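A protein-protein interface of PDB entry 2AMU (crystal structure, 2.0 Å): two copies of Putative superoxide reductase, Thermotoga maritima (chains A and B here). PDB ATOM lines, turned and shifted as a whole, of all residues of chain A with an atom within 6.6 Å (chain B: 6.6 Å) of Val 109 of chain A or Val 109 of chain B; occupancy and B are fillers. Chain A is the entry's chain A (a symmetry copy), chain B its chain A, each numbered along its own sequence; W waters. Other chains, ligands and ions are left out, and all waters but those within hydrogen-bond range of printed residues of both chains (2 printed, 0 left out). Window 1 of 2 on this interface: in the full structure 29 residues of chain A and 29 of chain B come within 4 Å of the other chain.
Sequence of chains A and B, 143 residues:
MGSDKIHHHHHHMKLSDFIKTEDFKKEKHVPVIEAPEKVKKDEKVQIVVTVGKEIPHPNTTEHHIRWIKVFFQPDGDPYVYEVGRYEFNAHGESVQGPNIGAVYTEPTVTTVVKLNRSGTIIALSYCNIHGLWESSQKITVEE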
ATOM      1  N   ILE A  47       3.642 -30.838  16.577  1.00  0.00           N
ATOM      2  CA  ILE A  47       4.993 -31.402  16.708  1.00  0.00           C
ATOM      3  C   ILE A  47       5.961 -30.427  15.987  1.00  0.00           C
ATOM      4  O   ILE A  47       5.835 -30.168  14.784  1.00  0.00           O
ATOM      5  CB  ILE A  47       5.083 -32.815  16.105  1.00  0.00           C
ATOM      6  CG1 ILE A  47       4.095 -33.802  16.798  1.00  0.00           C
ATOM      7  CG2 ILE A  47       6.532 -33.410  16.169  1.00  0.00           C
ATOM      8  CD1 ILE A  47       4.059 -35.219  16.122  1.00  0.00           C
ATOM      9  N   VAL A  48       6.896 -29.871  16.739  1.00  0.00           N
ATOM     10  CA  VAL A  48       7.909 -28.954  16.177  1.00  0.00           C
ATOM     11  C   VAL A  48       9.176 -29.777  16.170  1.00  0.00           C
ATOM     12  O   VAL A  48       9.425 -30.486  17.149  1.00  0.00           O
ATOM     13  CB  VAL A  48       8.067 -27.669  17.004  1.00  0.00           C
ATOM     14  CG1 VAL A  48       8.986 -26.653  16.273  1.00  0.00           C
ATOM     15  CG2 VAL A  48       6.726 -27.054  17.286  1.00  0.00           C
ATOM     16  N   VAL A  49       9.893 -29.795  15.033  1.00  0.00           N
ATOM     17  CA  VAL A  49      11.210 -30.453  14.923  1.00  0.00           C
ATOM     18  C   VAL A  49      12.180 -29.407  14.394  1.00  0.00           C
ATOM     19  O   VAL A  49      11.871 -28.730  13.409  1.00  0.00           O
ATOM     20  CB  VAL A  49      11.194 -31.700  14.012  1.00  0.00           C
ATOM     21  CG1 VAL A  49      12.534 -32.458  14.141  1.00  0.00           C
ATOM     22  CG2 VAL A  49      10.020 -32.621  14.389  1.00  0.00           C
ATOM     23  N   THR A  50      13.335 -29.248  15.061  1.00  0.00           N
ATOM     24  CA  THR A  50      14.337 -28.274  14.670  1.00  0.00           C
ATOM     25  C   THR A  50      15.703 -28.914  14.661  1.00  0.00           C
ATOM     26  O   THR A  50      16.048 -29.602  15.613  1.00  0.00           O
ATOM     27  CB  THR A  50      14.375 -27.114  15.680  1.00  0.00           C
ATOM     28  OG1 THR A  50      13.036 -26.676  15.828  1.00  0.00           O
ATOM     29  CG2 THR A  50      15.277 -25.928  15.216  1.00  0.00           C
ATOM     30  N   ILE A  68      13.777 -32.760   7.145  1.00  0.00           N
ATOM     31  CA  ILE A  68      13.387 -33.439   8.370  1.00  0.00           C
ATOM     32  C   ILE A  68      12.214 -34.365   7.987  1.00  0.00           C
ATOM     33  O   ILE A  68      11.363 -33.956   7.249  1.00  0.00           O
ATOM     34  CB  ILE A  68      12.889 -32.414   9.435  1.00  0.00           C
ATOM     35  CG1 ILE A  68      14.066 -31.724  10.092  1.00  0.00           C
ATOM     36  CG2 ILE A  68      11.976 -33.092  10.536  1.00  0.00           C
ATOM     37  CD1 ILE A  68      13.666 -30.555  10.986  1.00  0.00           C
ATOM     38  N   VAL A  70       9.370 -37.183   9.882  1.00  0.00           N
ATOM     39  CA  VAL A  70       8.806 -37.642  11.129  1.00  0.00           C
ATOM     40  C   VAL A  70       8.123 -38.982  10.889  1.00  0.00           C
ATOM     41  O   VAL A  70       7.378 -39.152   9.922  1.00  0.00           O
ATOM     42  CB  VAL A  70       7.779 -36.619  11.753  1.00  0.00           C
ATOM     43  CG1 VAL A  70       7.081 -37.258  13.046  1.00  0.00           C
ATOM     44  CG2 VAL A  70       8.486 -35.297  12.065  1.00  0.00           C
ATOM     45  N   TYR A  86       9.636 -33.136   5.215  1.00  0.00           N
ATOM     46  CA  TYR A  86       9.509 -31.681   5.183  1.00  0.00           C
ATOM     47  C   TYR A  86      10.808 -31.180   4.601  1.00  0.00           C
ATOM     48  O   TYR A  86      11.822 -31.268   5.238  1.00  0.00           O
ATOM     49  CB  TYR A  86       9.239 -31.160   6.619  1.00  0.00           C
ATOM     50  CG  TYR A  86       8.065 -31.898   7.266  1.00  0.00           C
ATOM     51  CD1 TYR A  86       6.759 -31.570   6.962  1.00  0.00           C
ATOM     52  CD2 TYR A  86       8.281 -32.991   8.125  1.00  0.00           C
ATOM     53  CE1 TYR A  86       5.694 -32.304   7.499  1.00  0.00           C
ATOM     54  CE2 TYR A  86       7.208 -33.706   8.694  1.00  0.00           C
ATOM     55  CZ  TYR A  86       5.938 -33.360   8.362  1.00  0.00           C
ATOM     56  OH  TYR A  86       4.910 -34.071   8.880  1.00  0.00           O
ATOM     57  N   PHE A  88      13.512 -28.607   2.960  1.00  0.00           N
ATOM     58  CA  PHE A  88      13.926 -27.215   3.044  1.00  0.00           C
ATOM     59  C   PHE A  88      14.835 -26.956   1.830  1.00  0.00           C
ATOM     60  O   PHE A  88      15.983 -27.400   1.814  1.00  0.00           O
ATOM     61  CB  PHE A  88      14.689 -26.970   4.372  1.00  0.00           C
ATOM     62  CG  PHE A  88      14.016 -27.601   5.590  1.00  0.00           C
ATOM     63  CD1 PHE A  88      12.735 -27.217   5.980  1.00  0.00           C
ATOM     64  CD2 PHE A  88      14.650 -28.612   6.307  1.00  0.00           C
ATOM     65  CE1 PHE A  88      12.100 -27.824   7.060  1.00  0.00           C
ATOM     66  CE2 PHE A  88      14.019 -29.206   7.381  1.00  0.00           C
ATOM     67  CZ  PHE A  88      12.748 -28.804   7.760  1.00  0.00           C
ATOM     68  N   GLU A 106      15.047 -22.425   6.653  1.00  0.00           N
ATOM     69  CA  GLU A 106      15.637 -22.887   7.912  1.00  0.00           C
ATOM     70  C   GLU A 106      15.101 -24.272   8.282  1.00  0.00           C
ATOM     71  O   GLU A 106      13.924 -24.603   7.964  1.00  0.00           O
ATOM     72  CB  GLU A 106      15.327 -21.845   9.011  1.00  0.00           C
ATOM     73  CG  GLU A 106      16.092 -20.553   8.801  1.00  0.00           C
ATOM     74  CD  GLU A 106      17.598 -20.830   8.831  1.00  0.00           C
ATOM     75  OE1 GLU A 106      18.106 -21.078   9.932  1.00  0.00           O
ATOM     76  OE2 GLU A 106      18.244 -20.880   7.771  1.00  0.00           O
ATOM     77  N   PRO A 107      15.953 -25.121   8.900  1.00  0.00           N
ATOM     78  CA  PRO A 107      15.523 -26.486   9.167  1.00  0.00           C
ATOM     79  C   PRO A 107      14.724 -26.601  10.484  1.00  0.00           C
ATOM     80  O   PRO A 107      15.160 -27.212  11.439  1.00  0.00           O
ATOM     81  CB  PRO A 107      16.831 -27.263   9.185  1.00  0.00           C
ATOM     82  CG  PRO A 107      17.841 -26.265   9.604  1.00  0.00           C
ATOM     83  CD  PRO A 107      17.339 -24.910   9.335  1.00  0.00           C
ATOM     84  N   THR A 108      13.553 -25.989  10.481  1.00  0.00           N
ATOM     85  CA  THR A 108      12.555 -26.144  11.540  1.00  0.00           C
ATOM     86  C   THR A 108      11.172 -26.289  10.863  1.00  0.00           C
ATOM     87  O   THR A 108      10.867 -25.652   9.821  1.00  0.00           O
ATOM     88  CB  THR A 108      12.603 -24.973  12.568  1.00  0.00           C
ATOM     89  OG1 THR A 108      11.559 -25.132  13.554  1.00  0.00           O
ATOM     90  CG2 THR A 108      12.432 -23.675  11.875  1.00  0.00           C
ATOM     91  N   VAL A 109      10.354 -27.168  11.419  1.00  0.00           N
ATOM     92  CA  VAL A 109       9.039 -27.383  10.849  1.00  0.00           C
ATOM     93  C   VAL A 109       8.043 -27.692  11.973  1.00  0.00           C
ATOM     94  O   VAL A 109       8.410 -28.309  12.962  1.00  0.00           O
ATOM     95  CB  VAL A 109       9.070 -28.469   9.777  1.00  0.00           C
ATOM     96  CG1 VAL A 109       9.436 -29.813  10.391  1.00  0.00           C
ATOM     97  CG2 VAL A 109       7.704 -28.553   9.053  1.00  0.00           C
ATOM     98  N   THR A 110       6.808 -27.200  11.827  1.00  0.00           N
ATOM     99  CA  THR A 110       5.709 -27.615  12.681  1.00  0.00           C
ATOM    100  C   THR A 110       4.741 -28.402  11.818  1.00  0.00           C
ATOM    101  O   THR A 110       4.231 -27.899  10.823  1.00  0.00           O
ATOM    102  CB  THR A 110       5.024 -26.445  13.386  1.00  0.00           C
ATOM    103  OG1 THR A 110       6.022 -25.656  14.052  1.00  0.00           O
ATOM    104  CG2 THR A 110       3.963 -26.948  14.402  1.00  0.00           C
ATOM    105  N   THR A 111       4.496 -29.639  12.239  1.00  0.00           N
ATOM    106  CA  THR A 111       3.508 -30.526  11.625  1.00  0.00           C
ATOM    107  C   THR A 111       2.396 -30.780  12.633  1.00  0.00           C
ATOM    108  O   THR A 111       2.589 -30.589  13.796  1.00  0.00           O
ATOM    109  CB  THR A 111       4.172 -31.829  11.107  1.00  0.00           C
ATOM    110  OG1 THR A 111       3.252 -32.528  10.261  1.00  0.00           O
ATOM    111  CG2 THR A 111       4.675 -32.735  12.262  1.00  0.00           C
ATOM    112  N   VAL A 112       1.204 -31.124  12.162  1.00  0.00           N
ATOM    113  CA  VAL A 112       0.062 -31.330  13.034  1.00  0.00           C
ATOM    114  C   VAL A 112      -0.511 -32.711  12.753  1.00  0.00           C
ATOM    115  O   VAL A 112      -0.787 -33.032  11.607  1.00  0.00           O
ATOM    116  CB  VAL A 112      -1.026 -30.286  12.815  1.00  0.00           C
ATOM    117  CG1 VAL A 112      -2.360 -30.681  13.617  1.00  0.00           C
ATOM    118  CG2 VAL A 112      -0.490 -28.867  13.171  1.00  0.00           C
ATOM    119  N   ILE B  47       6.030 -18.752   8.261  1.00  0.00           N
ATOM    120  CA  ILE B  47       4.982 -18.862   7.238  1.00  0.00           C
ATOM    121  C   ILE B  47       4.140 -20.118   7.586  1.00  0.00           C
ATOM    122  O   ILE B  47       4.654 -21.242   7.645  1.00  0.00           O
ATOM    123  CB  ILE B  47       5.576 -18.973   5.821  1.00  0.00           C
ATOM    124  CG1 ILE B  47       6.450 -17.734   5.464  1.00  0.00           C
ATOM    125  CG2 ILE B  47       4.480 -19.164   4.717  1.00  0.00           C
ATOM    126  CD1 ILE B  47       7.184 -17.870   4.083  1.00  0.00           C
ATOM    127  N   VAL B  48       2.861 -19.908   7.850  1.00  0.00           N
ATOM    128  CA  VAL B  48       1.934 -21.016   8.159  1.00  0.00           C
ATOM    129  C   VAL B  48       1.093 -21.141   6.910  1.00  0.00           C
ATOM    130  O   VAL B  48       0.699 -20.110   6.357  1.00  0.00           O
ATOM    131  CB  VAL B  48       1.074 -20.738   9.401  1.00  0.00           C
ATOM    132  CG1 VAL B  48       0.266 -22.001   9.806  1.00  0.00           C
ATOM    133  CG2 VAL B  48       1.932 -20.277  10.545  1.00  0.00           C
ATOM    134  N   VAL B  49       0.936 -22.372   6.393  1.00  0.00           N
ATOM    135  CA  VAL B  49       0.043 -22.657   5.253  1.00  0.00           C
ATOM    136  C   VAL B  49      -0.900 -23.765   5.701  1.00  0.00           C
ATOM    137  O   VAL B  49      -0.442 -24.773   6.248  1.00  0.00           O
ATOM    138  CB  VAL B  49       0.802 -23.066   3.971  1.00  0.00           C
ATOM    139  CG1 VAL B  49      -0.178 -23.112   2.777  1.00  0.00           C
ATOM    140  CG2 VAL B  49       1.944 -22.073   3.688  1.00  0.00           C
ATOM    141  N   THR B  50      -2.214 -23.569   5.503  1.00  0.00           N
ATOM    142  CA  THR B  50      -3.219 -24.539   5.900  1.00  0.00           C
ATOM    143  C   THR B  50      -4.200 -24.755   4.775  1.00  0.00           C
ATOM    144  O   THR B  50      -4.672 -23.784   4.198  1.00  0.00           O
ATOM    145  CB  THR B  50      -4.009 -24.019   7.113  1.00  0.00           C
ATOM    146  OG1 THR B  50      -3.045 -23.622   8.072  1.00  0.00           O
ATOM    147  CG2 THR B  50      -4.962 -25.093   7.727  1.00  0.00           C
ATOM    148  N   ILE B  68       1.655 -29.662   0.698  1.00  0.00           N
ATOM    149  CA  ILE B  68       1.706 -28.226   0.475  1.00  0.00           C
ATOM    150  C   ILE B  68       3.154 -27.913   0.046  1.00  0.00           C
ATOM    151  O   ILE B  68       4.061 -28.449   0.616  1.00  0.00           O
ATOM    152  CB  ILE B  68       1.396 -27.451   1.793  1.00  0.00           C
ATOM    153  CG1 ILE B  68      -0.094 -27.444   2.061  1.00  0.00           C
ATOM    154  CG2 ILE B  68       1.948 -25.969   1.759  1.00  0.00           C
ATOM    155  CD1 ILE B  68      -0.464 -26.899   3.437  1.00  0.00           C
ATOM    156  N   VAL B  70       5.704 -24.440  -0.982  1.00  0.00           N
ATOM    157  CA  VAL B  70       5.829 -23.003  -0.932  1.00  0.00           C
ATOM    158  C   VAL B  70       6.922 -22.577  -1.904  1.00  0.00           C
ATOM    159  O   VAL B  70       8.006 -23.162  -1.937  1.00  0.00           O
ATOM    160  CB  VAL B  70       6.153 -22.463   0.514  1.00  0.00           C
ATOM    161  CG1 VAL B  70       6.430 -20.885   0.464  1.00  0.00           C
ATOM    162  CG2 VAL B  70       5.016 -22.825   1.473  1.00  0.00           C
ATOM    163  N   TYR B  86       6.122 -30.012   1.665  1.00  0.00           N
ATOM    164  CA  TYR B  86       5.803 -30.473   3.015  1.00  0.00           C
ATOM    165  C   TYR B  86       4.763 -31.551   2.832  1.00  0.00           C
ATOM    166  O   TYR B  86       3.658 -31.259   2.465  1.00  0.00           O
ATOM    167  CB  TYR B  86       5.300 -29.272   3.859  1.00  0.00           C
ATOM    168  CG  TYR B  86       6.278 -28.097   3.791  1.00  0.00           C
ATOM    169  CD1 TYR B  86       7.428 -28.079   4.553  1.00  0.00           C
ATOM    170  CD2 TYR B  86       6.078 -27.040   2.885  1.00  0.00           C
ATOM    171  CE1 TYR B  86       8.356 -27.037   4.425  1.00  0.00           C
ATOM    172  CE2 TYR B  86       6.992 -25.972   2.782  1.00  0.00           C
ATOM    173  CZ  TYR B  86       8.118 -25.996   3.541  1.00  0.00           C
ATOM    174  OH  TYR B  86       9.014 -24.990   3.415  1.00  0.00           O
ATOM    175  N   PHE B  88       2.306 -34.675   3.743  1.00  0.00           N
ATOM    176  CA  PHE B  88       1.492 -35.175   4.841  1.00  0.00           C
ATOM    177  C   PHE B  88       1.117 -36.624   4.479  1.00  0.00           C
ATOM    178  O   PHE B  88       0.267 -36.843   3.617  1.00  0.00           O
ATOM    179  CB  PHE B  88       0.225 -34.296   5.002  1.00  0.00           C
ATOM    180  CG  PHE B  88       0.508 -32.796   4.934  1.00  0.00           C
ATOM    181  CD1 PHE B  88       1.340 -32.182   5.867  1.00  0.00           C
ATOM    182  CD2 PHE B  88      -0.022 -32.019   3.907  1.00  0.00           C
ATOM    183  CE1 PHE B  88       1.639 -30.824   5.780  1.00  0.00           C
ATOM    184  CE2 PHE B  88       0.272 -30.673   3.829  1.00  0.00           C
ATOM    185  CZ  PHE B  88       1.096 -30.077   4.772  1.00  0.00           C
ATOM    186  N   GLU B 106      -2.383 -33.831   9.357  1.00  0.00           N
ATOM    187  CA  GLU B 106      -3.258 -32.732   8.941  1.00  0.00           C
ATOM    188  C   GLU B 106      -2.523 -31.789   7.985  1.00  0.00           C
ATOM    189  O   GLU B 106      -1.279 -31.610   8.102  1.00  0.00           O
ATOM    190  CB  GLU B 106      -3.749 -31.990  10.205  1.00  0.00           C
ATOM    191  CG  GLU B 106      -4.718 -32.829  11.016  1.00  0.00           C
ATOM    192  CD  GLU B 106      -5.946 -33.169  10.168  1.00  0.00           C
ATOM    193  OE1 GLU B 106      -6.753 -32.257   9.947  1.00  0.00           O
ATOM    194  OE2 GLU B 106      -6.063 -34.299   9.665  1.00  0.00           O
ATOM    195  N   PRO B 107      -3.251 -31.220   6.997  1.00  0.00           N
ATOM    196  CA  PRO B 107      -2.572 -30.409   5.997  1.00  0.00           C
ATOM    197  C   PRO B 107      -2.377 -28.948   6.461  1.00  0.00           C
ATOM    198  O   PRO B 107      -2.951 -28.027   5.917  1.00  0.00           O
ATOM    199  CB  PRO B 107      -3.472 -30.539   4.777  1.00  0.00           C
ATOM    200  CG  PRO B 107      -4.816 -30.793   5.344  1.00  0.00           C
ATOM    201  CD  PRO B 107      -4.687 -31.319   6.710  1.00  0.00           C
ATOM    202  N   THR B 108      -1.550 -28.793   7.480  1.00  0.00           N
ATOM    203  CA  THR B 108      -1.067 -27.491   7.941  1.00  0.00           C
ATOM    204  C   THR B 108       0.444 -27.631   8.241  1.00  0.00           C
ATOM    205  O   THR B 108       0.933 -28.678   8.739  1.00  0.00           O
ATOM    206  CB  THR B 108      -1.878 -26.963   9.164  1.00  0.00           C
ATOM    207  OG1 THR B 108      -1.324 -25.711   9.625  1.00  0.00           O
ATOM    208  CG2 THR B 108      -1.845 -27.952  10.266  1.00  0.00           C
ATOM    209  N   VAL B 109       1.194 -26.600   7.886  1.00  0.00           N
ATOM    210  CA  VAL B 109       2.624 -26.642   8.116  1.00  0.00           C
ATOM    211  C   VAL B 109       3.126 -25.232   8.449  1.00  0.00           C
ATOM    212  O   VAL B 109       2.599 -24.258   7.934  1.00  0.00           O
ATOM    213  CB  VAL B 109       3.359 -27.261   6.929  1.00  0.00           C
ATOM    214  CG1 VAL B 109       3.204 -26.387   5.692  1.00  0.00           C
ATOM    215  CG2 VAL B 109       4.855 -27.468   7.268  1.00  0.00           C
ATOM    216  N   THR B 110       4.102 -25.147   9.360  1.00  0.00           N
ATOM    217  CA  THR B 110       4.833 -23.914   9.590  1.00  0.00           C
ATOM    218  C   THR B 110       6.256 -24.139   9.113  1.00  0.00           C
ATOM    219  O   THR B 110       6.943 -25.038   9.583  1.00  0.00           O
ATOM    220  CB  THR B 110       4.786 -23.452  11.045  1.00  0.00           C
ATOM    221  OG1 THR B 110       3.417 -23.413  11.476  1.00  0.00           O
ATOM    222  CG2 THR B 110       5.447 -22.057  11.212  1.00  0.00           C
ATOM    223  N   THR B 111       6.674 -23.287   8.181  1.00  0.00           N
ATOM    224  CA  THR B 111       8.044 -23.250   7.669  1.00  0.00           C
ATOM    225  C   THR B 111       8.675 -21.926   8.077  1.00  0.00           C
ATOM    226  O   THR B 111       7.983 -21.005   8.388  1.00  0.00           O
ATOM    227  CB  THR B 111       8.074 -23.495   6.137  1.00  0.00           C
ATOM    228  OG1 THR B 111       9.421 -23.748   5.723  1.00  0.00           O
ATOM    229  CG2 THR B 111       7.450 -22.319   5.339  1.00  0.00           C
ATOM    230  N   VAL B 112       9.999 -21.876   8.160  1.00  0.00           N
ATOM    231  CA  VAL B 112      10.697 -20.681   8.598  1.00  0.00           C
ATOM    232  C   VAL B 112      11.724 -20.312   7.538  1.00  0.00           C
ATOM    233  O   VAL B 112      12.521 -21.151   7.148  1.00  0.00           O
ATOM    234  CB  VAL B 112      11.408 -20.884   9.931  1.00  0.00           C
ATOM    235  CG1 VAL B 112      12.357 -19.633  10.263  1.00  0.00           C
ATOM    236  CG2 VAL B 112      10.371 -21.186  11.054  1.00  0.00           C
HETATM  237  O   HOH W   1      11.229 -24.408   7.538  1.00  0.00           O
HETATM  238  O   HOH W   2       1.161 -31.236   9.282  1.00  0.00           O
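The backbone NH (N) of Glu 106 of chain B lies within hydrogen-bond range of the backbone carbonyl oxygen (O) of Val 112 of chain A (2.9 Å). The backbone NH of Thr 110 of chain B is in hydrogen-bond range of the backbone carbonyl oxygen of Thr 110 of chain A. The backbone carbonyl oxygen (O) of Val 112 of chain B sits at hydrogen-bond distance from the backbone NH (N) of Glu 106 of chain A (2.9 Å).
The backbone carbonyl oxygen (O) of Val 109 of chain B is in hydrogen-bond range of the backbone NH (N) of Val 49 of chain B (2.9 Å). The side-chain hydroxyl (OG1) of Thr 50 of chain B sits at hydrogen-bond distance from the side-chain hydroxyl (OG1) of Thr 108 of chain B, at 3.1 Å. The backbone carbonyl oxygen (O) of Val 109 of chain A sits at hydrogen-bond distance from the backbone NH (N) of Val 49 of chain A. The side-chain hydroxyl (OG1) of Thr 50 of chain A sits at hydrogen-bond distance from the side-chain hydroxyl (OG1) of Thr 108 of chain A (3.1 Å).
Among the printed residues, pairs that only touch across the chains: Val 112 of chain A with Thr 108 of chain B (3.3 Å), Thr 108 of chain A with Val 112 of chain B (3.3 Å), Thr 110 of chain A with Val 109 of chain B (3.4 Å), Val 109 of chain A with Thr 110 of chain B (3.4 Å), Val 109 of chain A with Val 109 of chain B (3.5 Å), Thr 110 of chain A with Thr 108 of chain B (3.98 Å) and Thr 108 of chain A with Thr 110 of chain B (3.98 Å).
Of the printed residues of chain B, Val 109 of chain A touches Val 109 and Thr 110. Printed residues of chain B within 4 Å of Thr 110 of chain A: Thr 108 (3.98 Å), Val 109 (3.4 Å) and Thr 110 (3.1 Å). Printed residues of chain B within 4 Å of Val 112 of chain A: Glu 106 (2.9 Å) and Thr 108 (3.3 Å). Val 109 of chain B touches two residues of chain A. Of the printed residues of chain A, Thr 110 of chain B touches Thr 108, Val 109 and Thr 110. The nearest residue of chain B that does not touch Val 109 of chain A is Tyr 86 of chain B (4.5 Å). The nearest residue of chain A that does not touch Val 109 of chain B is Tyr 86 of chain A (4.5 Å). The nearest printed residue of chain B that does not touch Thr 110 of chain A is Thr 111 of chain B (5.4 Å).
Of the 15 printed residues of chain A, 5 touch a printed residue of chain B. Hydrophobic or aromatic side chains of chain B that line the printed part of chain A: Val 109 and Val 112. Among the printed residues, 10 pairs touch across the chains.
Glu 106 of chain A touches Val 112 of chain B, and with the chains exchanged Val 112 of chain A touches Glu 106 of chain B. Thr 108 of chain A touches Thr 110 of chain B, and with the chains exchanged Thr 110 of chain A touches Thr 108 of chain B. Thr 108 of chain A touches Val 112 of chain B, and with the chains exchanged Val 112 of chain A touches Thr 108 of chain B. Val 109 of chain A touches its own counterpart, Val 109 of chain B. Of the 10 pairs that touch across the chains among the printed residues, 10 have their exchanged pair printed and touching as well.
Water W2 lies within hydrogen-bond range of the backbone carbonyl oxygen (O) of Thr 108 of chain B (2.6 Å), the side-chain hydroxyl (OG1) of Thr 111 of chain A (2.6 Å), the backbone carbonyl oxygen (O) of Glu 106 of chain B (2.7 Å) and the backbone NH (N) of Val 112 of chain A (2.9 Å). Water W1 lies within hydrogen-bond range of O of Thr 108 of chain A (2.6 Å), OG1 of Thr 111 of chain B (2.6 Å), O of Glu 106 of chain A (2.7 Å) and N of Val 112 of chain B (2.9 Å).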
